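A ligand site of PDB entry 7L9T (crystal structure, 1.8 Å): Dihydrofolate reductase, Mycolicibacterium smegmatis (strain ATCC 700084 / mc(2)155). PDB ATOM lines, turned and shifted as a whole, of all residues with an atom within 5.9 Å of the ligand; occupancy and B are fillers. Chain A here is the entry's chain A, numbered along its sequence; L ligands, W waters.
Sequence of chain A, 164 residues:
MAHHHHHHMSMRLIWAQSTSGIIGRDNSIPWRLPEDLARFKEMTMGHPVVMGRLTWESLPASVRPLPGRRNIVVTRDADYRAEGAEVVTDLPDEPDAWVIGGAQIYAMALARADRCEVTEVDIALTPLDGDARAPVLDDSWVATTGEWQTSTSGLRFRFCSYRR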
ATOM      1  N   ILE A  14     -15.060  19.974 -12.118  1.00  0.00           N
ATOM      2  CA  ILE A  14     -15.155  20.030 -10.659  1.00  0.00           C
ATOM      3  C   ILE A  14     -15.589  21.426 -10.250  1.00  0.00           C
ATOM      4  O   ILE A  14     -15.052  22.421 -10.749  1.00  0.00           O
ATOM      5  CB  ILE A  14     -13.827  19.596 -10.002  1.00  0.00           C
ATOM      6  CG1 ILE A  14     -13.983  19.512  -8.487  1.00  0.00           C
ATOM      7  CG2 ILE A  14     -12.675  20.516 -10.413  1.00  0.00           C
ATOM      8  CD1 ILE A  14     -12.805  18.790  -7.804  1.00  0.00           C
ATOM      9  N   TRP A  15     -16.593  21.512  -9.386  1.00  0.00           N
ATOM     10  CA  TRP A  15     -17.083  22.806  -8.946  1.00  0.00           C
ATOM     11  C   TRP A  15     -17.694  22.669  -7.564  1.00  0.00           C
ATOM     12  O   TRP A  15     -18.025  21.569  -7.111  1.00  0.00           O
ATOM     13  CB  TRP A  15     -18.108  23.411  -9.929  1.00  0.00           C
ATOM     14  CG  TRP A  15     -19.472  22.724 -10.006  1.00  0.00           C
ATOM     15  CD1 TRP A  15     -20.538  22.894  -9.169  1.00  0.00           C
ATOM     16  CD2 TRP A  15     -19.906  21.795 -11.024  1.00  0.00           C
ATOM     17  NE1 TRP A  15     -21.602  22.111  -9.574  1.00  0.00           N
ATOM     18  CE2 TRP A  15     -21.235  21.431 -10.717  1.00  0.00           C
ATOM     19  CE3 TRP A  15     -19.287  21.230 -12.150  1.00  0.00           C
ATOM     20  CZ2 TRP A  15     -21.964  20.535 -11.501  1.00  0.00           C
ATOM     21  CZ3 TRP A  15     -20.022  20.335 -12.921  1.00  0.00           C
ATOM     22  CH2 TRP A  15     -21.340  19.996 -12.595  1.00  0.00           C
ATOM     23  N   ALA A  16     -17.849  23.810  -6.902  1.00  0.00           N
ATOM     24  CA  ALA A  16     -18.608  23.892  -5.665  1.00  0.00           C
ATOM     25  C   ALA A  16     -19.778  24.835  -5.903  1.00  0.00           C
ATOM     26  O   ALA A  16     -19.627  25.861  -6.556  1.00  0.00           O
ATOM     27  CB  ALA A  16     -17.733  24.412  -4.500  1.00  0.00           C
ATOM     28  N   ASP A  36     -13.594  21.317   1.225  1.00  0.00           N
ATOM     29  CA  ASP A  36     -13.695  21.404  -0.243  1.00  0.00           C
ATOM     30  C   ASP A  36     -12.351  21.718  -0.883  1.00  0.00           C
ATOM     31  O   ASP A  36     -12.028  21.175  -1.944  1.00  0.00           O
ATOM     32  CB  ASP A  36     -14.706  22.469  -0.651  1.00  0.00           C
ATOM     33  CG  ASP A  36     -14.705  22.681  -2.151  1.00  0.00           C
ATOM     34  OD1 ASP A  36     -15.139  21.753  -2.855  1.00  0.00           O
ATOM     35  OD2 ASP A  36     -14.227  23.731  -2.616  1.00  0.00           O
ATOM     36  N   LEU A  37     -11.550  22.592  -0.258  1.00  0.00           N
ATOM     37  CA  LEU A  37     -10.204  22.830  -0.784  1.00  0.00           C
ATOM     38  C   LEU A  37      -9.400  21.541  -0.774  1.00  0.00           C
ATOM     39  O   LEU A  37      -8.678  21.244  -1.731  1.00  0.00           O
ATOM     40  CB  LEU A  37      -9.469  23.887   0.033  1.00  0.00           C
ATOM     41  CG  LEU A  37      -9.707  25.358  -0.348  1.00  0.00           C
ATOM     42  CD1 LEU A  37     -11.173  25.692  -0.373  1.00  0.00           C
ATOM     43  CD2 LEU A  37      -8.979  26.286   0.626  1.00  0.00           C
ATOM     44  N   PHE A  40     -10.602  19.296  -3.604  1.00  0.00           N
ATOM     45  CA  PHE A  40     -10.194  19.862  -4.880  1.00  0.00           C
ATOM     46  C   PHE A  40      -8.725  19.548  -5.161  1.00  0.00           C
ATOM     47  O   PHE A  40      -8.375  19.141  -6.264  1.00  0.00           O
ATOM     48  CB  PHE A  40     -10.419  21.371  -4.880  1.00  0.00           C
ATOM     49  CG  PHE A  40      -9.869  22.079  -6.096  1.00  0.00           C
ATOM     50  CD1 PHE A  40     -10.641  22.197  -7.248  1.00  0.00           C
ATOM     51  CD2 PHE A  40      -8.596  22.622  -6.083  1.00  0.00           C
ATOM     52  CE1 PHE A  40     -10.152  22.853  -8.371  1.00  0.00           C
ATOM     53  CE2 PHE A  40      -8.080  23.283  -7.207  1.00  0.00           C
ATOM     54  CZ  PHE A  40      -8.865  23.391  -8.366  1.00  0.00           C
ATOM     55  N   LYS A  41      -7.858  19.760  -4.166  1.00  0.00           N
ATOM     56  CA  LYS A  41      -6.436  19.474  -4.306  1.00  0.00           C
ATOM     57  C   LYS A  41      -6.194  18.000  -4.584  1.00  0.00           C
ATOM     58  O   LYS A  41      -5.350  17.645  -5.412  1.00  0.00           O
ATOM     59  CB  LYS A  41      -5.686  19.903  -3.028  1.00  0.00           C
ATOM     60  CG  LYS A  41      -4.179  19.731  -3.072  1.00  0.00           C
ATOM     61  CD  LYS A  41      -3.572  20.236  -1.750  1.00  0.00           C
ATOM     62  CE  LYS A  41      -2.070  20.107  -1.737  1.00  0.00           C
ATOM     63  NZ  LYS A  41      -1.510  20.685  -0.474  1.00  0.00           N
ATOM     64  N   THR A  44      -7.321  17.199  -8.334  1.00  0.00           N
ATOM     65  CA  THR A  44      -6.659  17.856  -9.460  1.00  0.00           C
ATOM     66  C   THR A  44      -5.138  17.736  -9.454  1.00  0.00           C
ATOM     67  O   THR A  44      -4.528  17.963 -10.501  1.00  0.00           O
ATOM     68  CB  THR A  44      -7.014  19.344  -9.503  1.00  0.00           C
ATOM     69  OG1 THR A  44      -6.562  19.970  -8.295  1.00  0.00           O
ATOM     70  CG2 THR A  44      -8.502  19.529  -9.652  1.00  0.00           C
ATOM     71  N   MET A  45      -4.505  17.405  -8.327  1.00  0.00           N
ATOM     72  CA  MET A  45      -3.048  17.402  -8.280  1.00  0.00           C
ATOM     73  C   MET A  45      -2.440  16.460  -9.319  1.00  0.00           C
ATOM     74  O   MET A  45      -2.886  15.320  -9.472  1.00  0.00           O
ATOM     75  CB  MET A  45      -2.553  16.989  -6.886  1.00  0.00           C
ATOM     76  CG  MET A  45      -1.038  17.058  -6.744  1.00  0.00           C
ATOM     77  SD  MET A  45      -0.463  18.754  -6.951  1.00  0.00           S
ATOM     78  CE  MET A  45      -1.414  19.612  -5.691  1.00  0.00           C
ATOM     79  N   THR A  55     -11.326  33.224 -13.229  1.00  0.00           N
ATOM     80  CA  THR A  55     -10.909  32.222 -12.258  1.00  0.00           C
ATOM     81  C   THR A  55      -9.419  32.326 -11.965  1.00  0.00           C
ATOM     82  O   THR A  55      -9.006  32.272 -10.802  1.00  0.00           O
ATOM     83  CB  THR A  55     -11.240  30.812 -12.786  1.00  0.00           C
ATOM     84  OG1 THR A  55     -12.652  30.688 -12.954  1.00  0.00           O
ATOM     85  CG2 THR A  55     -10.756  29.764 -11.814  1.00  0.00           C
ATOM     86  N   LEU A  59      -7.585  33.324  -8.190  1.00  0.00           N
ATOM     87  CA  LEU A  59      -6.787  32.418  -7.374  1.00  0.00           C
ATOM     88  C   LEU A  59      -5.999  33.217  -6.337  1.00  0.00           C
ATOM     89  O   LEU A  59      -5.447  34.276  -6.650  1.00  0.00           O
ATOM     90  CB  LEU A  59      -5.821  31.626  -8.239  1.00  0.00           C
ATOM     91  CG  LEU A  59      -6.391  30.622  -9.240  1.00  0.00           C
ATOM     92  CD1 LEU A  59      -5.284  30.152 -10.157  1.00  0.00           C
ATOM     93  CD2 LEU A  59      -7.003  29.443  -8.502  1.00  0.00           C
ATOM     94  N   PRO A  60      -5.920  32.732  -5.092  1.00  0.00           N
ATOM     95  CA  PRO A  60      -4.991  33.344  -4.127  1.00  0.00           C
ATOM     96  C   PRO A  60      -3.601  33.408  -4.737  1.00  0.00           C
ATOM     97  O   PRO A  60      -3.169  32.489  -5.438  1.00  0.00           O
ATOM     98  CB  PRO A  60      -5.054  32.401  -2.920  1.00  0.00           C
ATOM     99  CG  PRO A  60      -6.377  31.712  -3.048  1.00  0.00           C
ATOM    100  CD  PRO A  60      -6.561  31.522  -4.535  1.00  0.00           C
ATOM    101  N   VAL A  63      -1.105  30.578  -4.737  1.00  0.00           N
ATOM    102  CA  VAL A  63      -1.309  29.399  -5.562  1.00  0.00           C
ATOM    103  C   VAL A  63      -1.752  29.802  -6.967  1.00  0.00           C
ATOM    104  O   VAL A  63      -2.602  29.139  -7.578  1.00  0.00           O
ATOM    105  CB  VAL A  63      -2.332  28.428  -4.923  1.00  0.00           C
ATOM    106  CG1 VAL A  63      -1.729  27.772  -3.708  1.00  0.00           C
ATOM    107  CG2 VAL A  63      -3.626  29.156  -4.564  1.00  0.00           C
ATOM    108  N   LEU A  66      -1.674  27.248  -9.753  1.00  0.00           N
ATOM    109  CA  LEU A  66      -1.905  26.149  -8.820  1.00  0.00           C
ATOM    110  C   LEU A  66      -0.730  25.173  -8.907  1.00  0.00           C
ATOM    111  O   LEU A  66      -0.465  24.653 -10.002  1.00  0.00           O
ATOM    112  CB  LEU A  66      -3.223  25.433  -9.142  1.00  0.00           C
ATOM    113  CG  LEU A  66      -4.469  26.282  -8.805  1.00  0.00           C
ATOM    114  CD1 LEU A  66      -5.693  25.748  -9.526  1.00  0.00           C
ATOM    115  CD2 LEU A  66      -4.722  26.314  -7.299  1.00  0.00           C
ATOM    116  N   PRO A  67      -0.008  24.920  -7.821  1.00  0.00           N
ATOM    117  CA  PRO A  67       1.241  24.144  -7.924  1.00  0.00           C
ATOM    118  C   PRO A  67       0.982  22.672  -8.220  1.00  0.00           C
ATOM    119  O   PRO A  67      -0.048  22.103  -7.849  1.00  0.00           O
ATOM    120  CB  PRO A  67       1.899  24.344  -6.555  1.00  0.00           C
ATOM    121  CG  PRO A  67       0.755  24.646  -5.623  1.00  0.00           C
ATOM    122  CD  PRO A  67      -0.259  25.394  -6.447  1.00  0.00           C
ATOM    123  N   ARG A  69       0.289  21.333 -10.973  1.00  0.00           N
ATOM    124  CA  ARG A  69      -0.685  21.162 -12.031  1.00  0.00           C
ATOM    125  C   ARG A  69      -0.315  22.070 -13.181  1.00  0.00           C
ATOM    126  O   ARG A  69       0.138  23.196 -12.967  1.00  0.00           O
ATOM    127  CB  ARG A  69      -2.096  21.493 -11.502  1.00  0.00           C
ATOM    128  CG  ARG A  69      -2.638  20.427 -10.578  1.00  0.00           C
ATOM    129  CD  ARG A  69      -3.601  21.011  -9.541  1.00  0.00           C
ATOM    130  NE  ARG A  69      -2.891  21.708  -8.478  1.00  0.00           N
ATOM    131  CZ  ARG A  69      -3.463  22.169  -7.378  1.00  0.00           C
ATOM    132  NH1 ARG A  69      -4.773  22.067  -7.181  1.00  0.00           N
ATOM    133  NH2 ARG A  69      -2.696  22.749  -6.448  1.00  0.00           N
ATOM    134  N   VAL A  99     -11.481  20.736 -15.517  1.00  0.00           N
ATOM    135  CA  VAL A  99     -12.014  22.074 -15.750  1.00  0.00           C
ATOM    136  C   VAL A  99     -12.499  22.624 -14.405  1.00  0.00           C
ATOM    137  O   VAL A  99     -13.314  21.998 -13.728  1.00  0.00           O
ATOM    138  CB  VAL A  99     -13.148  22.054 -16.790  1.00  0.00           C
ATOM    139  CG1 VAL A  99     -13.753  23.433 -16.914  1.00  0.00           C
ATOM    140  CG2 VAL A  99     -12.611  21.570 -18.139  1.00  0.00           C
ATOM    141  N   ILE A 100     -11.976  23.789 -14.013  1.00  0.00           N
ATOM    142  CA  ILE A 100     -12.118  24.263 -12.637  1.00  0.00           C
ATOM    143  C   ILE A 100     -12.770  25.628 -12.542  1.00  0.00           C
ATOM    144  O   ILE A 100     -12.866  26.172 -11.432  1.00  0.00           O
ATOM    145  CB  ILE A 100     -10.751  24.307 -11.919  1.00  0.00           C
ATOM    146  CG1 ILE A 100      -9.886  25.428 -12.523  1.00  0.00           C
ATOM    147  CG2 ILE A 100     -10.072  22.936 -11.958  1.00  0.00           C
ATOM    148  CD1 ILE A 100      -8.656  25.788 -11.697  1.00  0.00           C
ATOM    149  N   GLY A 101     -13.205  26.210 -13.634  1.00  0.00           N
ATOM    150  CA  GLY A 101     -13.789  27.523 -13.440  1.00  0.00           C
ATOM    151  C   GLY A 101     -14.077  28.246 -14.711  1.00  0.00           C
ATOM    152  O   GLY A 101     -13.340  28.117 -15.689  1.00  0.00           O
ATOM    153  N   TYR A 106     -17.453  25.505 -17.986  1.00  0.00           N
ATOM    154  CA  TYR A 106     -18.206  24.284 -17.704  1.00  0.00           C
ATOM    155  C   TYR A 106     -19.188  23.986 -18.832  1.00  0.00           C
ATOM    156  O   TYR A 106     -19.275  22.848 -19.309  1.00  0.00           O
ATOM    157  CB  TYR A 106     -18.945  24.405 -16.372  1.00  0.00           C
ATOM    158  CG  TYR A 106     -18.074  24.540 -15.140  1.00  0.00           C
ATOM    159  CD1 TYR A 106     -16.979  23.707 -14.932  1.00  0.00           C
ATOM    160  CD2 TYR A 106     -18.360  25.511 -14.174  1.00  0.00           C
ATOM    161  CE1 TYR A 106     -16.182  23.852 -13.796  1.00  0.00           C
ATOM    162  CE2 TYR A 106     -17.577  25.653 -13.037  1.00  0.00           C
ATOM    163  CZ  TYR A 106     -16.506  24.822 -12.850  1.00  0.00           C
ATOM    164  OH  TYR A 106     -15.716  24.962 -11.726  1.00  0.00           O
ATOM    165  N   GLU A 117     -17.320  16.245 -10.477  1.00  0.00           N
ATOM    166  CA  GLU A 117     -17.164  16.163  -9.037  1.00  0.00           C
ATOM    167  C   GLU A 117     -17.707  17.449  -8.448  1.00  0.00           C
ATOM    168  O   GLU A 117     -17.219  18.539  -8.758  1.00  0.00           O
ATOM    169  CB  GLU A 117     -15.702  15.971  -8.660  1.00  0.00           C
ATOM    170  CG  GLU A 117     -15.147  14.659  -9.159  1.00  0.00           C
ATOM    171  CD  GLU A 117     -15.760  13.474  -8.445  1.00  0.00           C
ATOM    172  OE1 GLU A 117     -16.231  13.635  -7.297  1.00  0.00           O
ATOM    173  OE2 GLU A 117     -15.766  12.368  -9.019  1.00  0.00           O
ATOM    174  N   VAL A 118     -18.729  17.333  -7.602  1.00  0.00           N
ATOM    175  CA  VAL A 118     -19.473  18.494  -7.129  1.00  0.00           C
ATOM    176  C   VAL A 118     -19.437  18.531  -5.614  1.00  0.00           C
ATOM    177  O   VAL A 118     -19.645  17.509  -4.944  1.00  0.00           O
ATOM    178  CB  VAL A 118     -20.929  18.444  -7.612  1.00  0.00           C
ATOM    179  CG1 VAL A 118     -21.736  19.666  -7.051  1.00  0.00           C
ATOM    180  CG2 VAL A 118     -20.967  18.385  -9.117  1.00  0.00           C
ATOM    181  N   THR A 119     -19.213  19.729  -5.063  1.00  0.00           N
ATOM    182  CA  THR A 119     -19.458  20.012  -3.655  1.00  0.00           C
ATOM    183  C   THR A 119     -20.705  20.871  -3.585  1.00  0.00           C
ATOM    184  O   THR A 119     -20.787  21.896  -4.258  1.00  0.00           O
ATOM    185  CB  THR A 119     -18.268  20.745  -3.040  1.00  0.00           C
ATOM    186  OG1 THR A 119     -17.078  19.974  -3.248  1.00  0.00           O
ATOM    187  CG2 THR A 119     -18.510  21.012  -1.524  1.00  0.00           C
HETATM  188  C1  LIG L   1      -8.547  28.517  -4.397  1.00  0.00           C
HETATM  189  C2  LIG L   1      -7.991  28.542  -3.135  1.00  0.00           C
HETATM  190  C3  LIG L   1      -6.336  25.111  -2.941  1.00  0.00           C
HETATM  191  C4  LIG L   1      -4.899  25.116  -3.463  1.00  0.00           C
HETATM  192  C5  LIG L   1     -11.264  25.406  -4.162  1.00  0.00           C
HETATM  193  C6  LIG L   1     -12.583  25.973  -4.726  1.00  0.00           C
HETATM  194  C7  LIG L   1     -13.123  24.990  -5.745  1.00  0.00           C
HETATM  195  C8  LIG L   1     -13.008  25.197  -7.087  1.00  0.00           C
HETATM  196  C9  LIG L   1     -10.970  26.237  -7.917  1.00  0.00           C
HETATM  197  C10 LIG L   1     -10.547  27.685  -8.111  1.00  0.00           C
HETATM  198  C11 LIG L   1     -10.060  28.284  -6.792  1.00  0.00           C
HETATM  199  C12 LIG L   1      -8.376  27.394  -5.181  1.00  0.00           C
HETATM  200  C13 LIG L   1      -7.266  27.458  -2.643  1.00  0.00           C
HETATM  201  C14 LIG L   1      -7.100  26.321  -3.428  1.00  0.00           C
HETATM  202  C15 LIG L   1      -4.519  23.730  -4.088  1.00  0.00           C
HETATM  203  C16 LIG L   1      -7.658  26.306  -4.701  1.00  0.00           C
HETATM  204  C17 LIG L   1     -13.544  24.217  -7.944  1.00  0.00           C
HETATM  205  C18 LIG L   1     -14.216  23.008  -6.113  1.00  0.00           C
HETATM  206  N1  LIG L   1     -13.458  24.359  -9.277  1.00  0.00           N
HETATM  207  N2  LIG L   1     -14.141  23.131  -7.442  1.00  0.00           N
HETATM  208  N3  LIG L   1     -14.821  21.923  -5.599  1.00  0.00           N
HETATM  209  N4  LIG L   1     -13.729  23.901  -5.272  1.00  0.00           N
HETATM  210  O1  LIG L   1     -12.397  26.318  -7.610  1.00  0.00           O
HETATM  211  O2  LIG L   1      -8.953  27.437  -6.446  1.00  0.00           O
HETATM  212  O3  LIG L   1      -5.464  23.077  -4.590  1.00  0.00           O
HETATM  213  O4  LIG L   1      -3.305  23.448  -3.994  1.00  0.00           O
HETATM  214  O   HOH W   1     -16.133  19.189  -5.794  1.00  0.00           O
HETATM  215  O   HOH W   2     -16.389  25.965  -7.995  1.00  0.00           O
HETATM  216  O   HOH W   3     -15.313  27.458  -4.918  1.00  0.00           O
HETATM  217  O   HOH W   4      -1.666  24.190  -2.131  1.00  0.00           O
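The guanidinium group (NE) of Arg 69 is in hydrogen-bond range of the backbone carbonyl oxygen (O) of Pro 67, at 2.9 Å. The side-chain hydroxyl of Tyr 106 is in hydrogen-bond range of the backbone carbonyl oxygen of Ile 100 (3.1 Å). O of Ile 14 lies within hydrogen-bond range of OH of Tyr 106 (2.8 Å). The backbone carbonyl oxygen (O) of Val 99 is in hydrogen-bond range of the backbone NH (N) of Ile 14, 3.1 Å away. The backbone carbonyl oxygen (O) of Trp 15 lies within hydrogen-bond range of the backbone NH (N) of Thr 119 (3.0 Å). N of Trp 15 lies within hydrogen-bond range of O of Glu 117 (3.1 Å). OH of Tyr 106 lies within hydrogen-bond range of N of Gly 101 (3.4 Å). The side-chain hydroxyl (OG1) of Thr 44 lies within hydrogen-bond range of the backbone carbonyl oxygen (O) of Phe 40 (2.8 Å).
Trp 15 touches the ligand. Ala 16 touches the ligand (N to N3, 3.8 Å). CD1 of Leu 37 touches C5 of the ligand, at 3.8 Å. Phe 40 touches the ligand. CB of Lys 41 touches O3 of the ligand (3.5 Å). Leu 59 touches the ligand. CG of Pro 60 touches C2 of the ligand, 3.6 Å away. CD2 of Leu 66 touches C16 of the ligand (3.9 Å). Thr 119 touches the ligand.
O4 of the ligand is in salt-bridge range of NH2 of Arg 69, 2.6 Å away. OD2 of Asp 36 is in hydrogen-bond range of N4 of the ligand (2.7 Å). A nitrogen (N1) of the ligand lies within hydrogen-bond range of the backbone carbonyl oxygen of Ile 100, 2.9 Å away. N1 of the ligand lies within hydrogen-bond range of O of Ile 14 (2.9 Å). N1 of the ligand sits at hydrogen-bond distance from OH of Tyr 106.
Water W1 lies within hydrogen-bond range of the side-chain hydroxyl of Thr 119 (2.8 Å), a nitrogen (N3) of the ligand (3.0 Å), the backbone carbonyl oxygen of Glu 117 (3.2 Å) and the backbone carbonyl oxygen of Trp 15 (3.3 Å).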
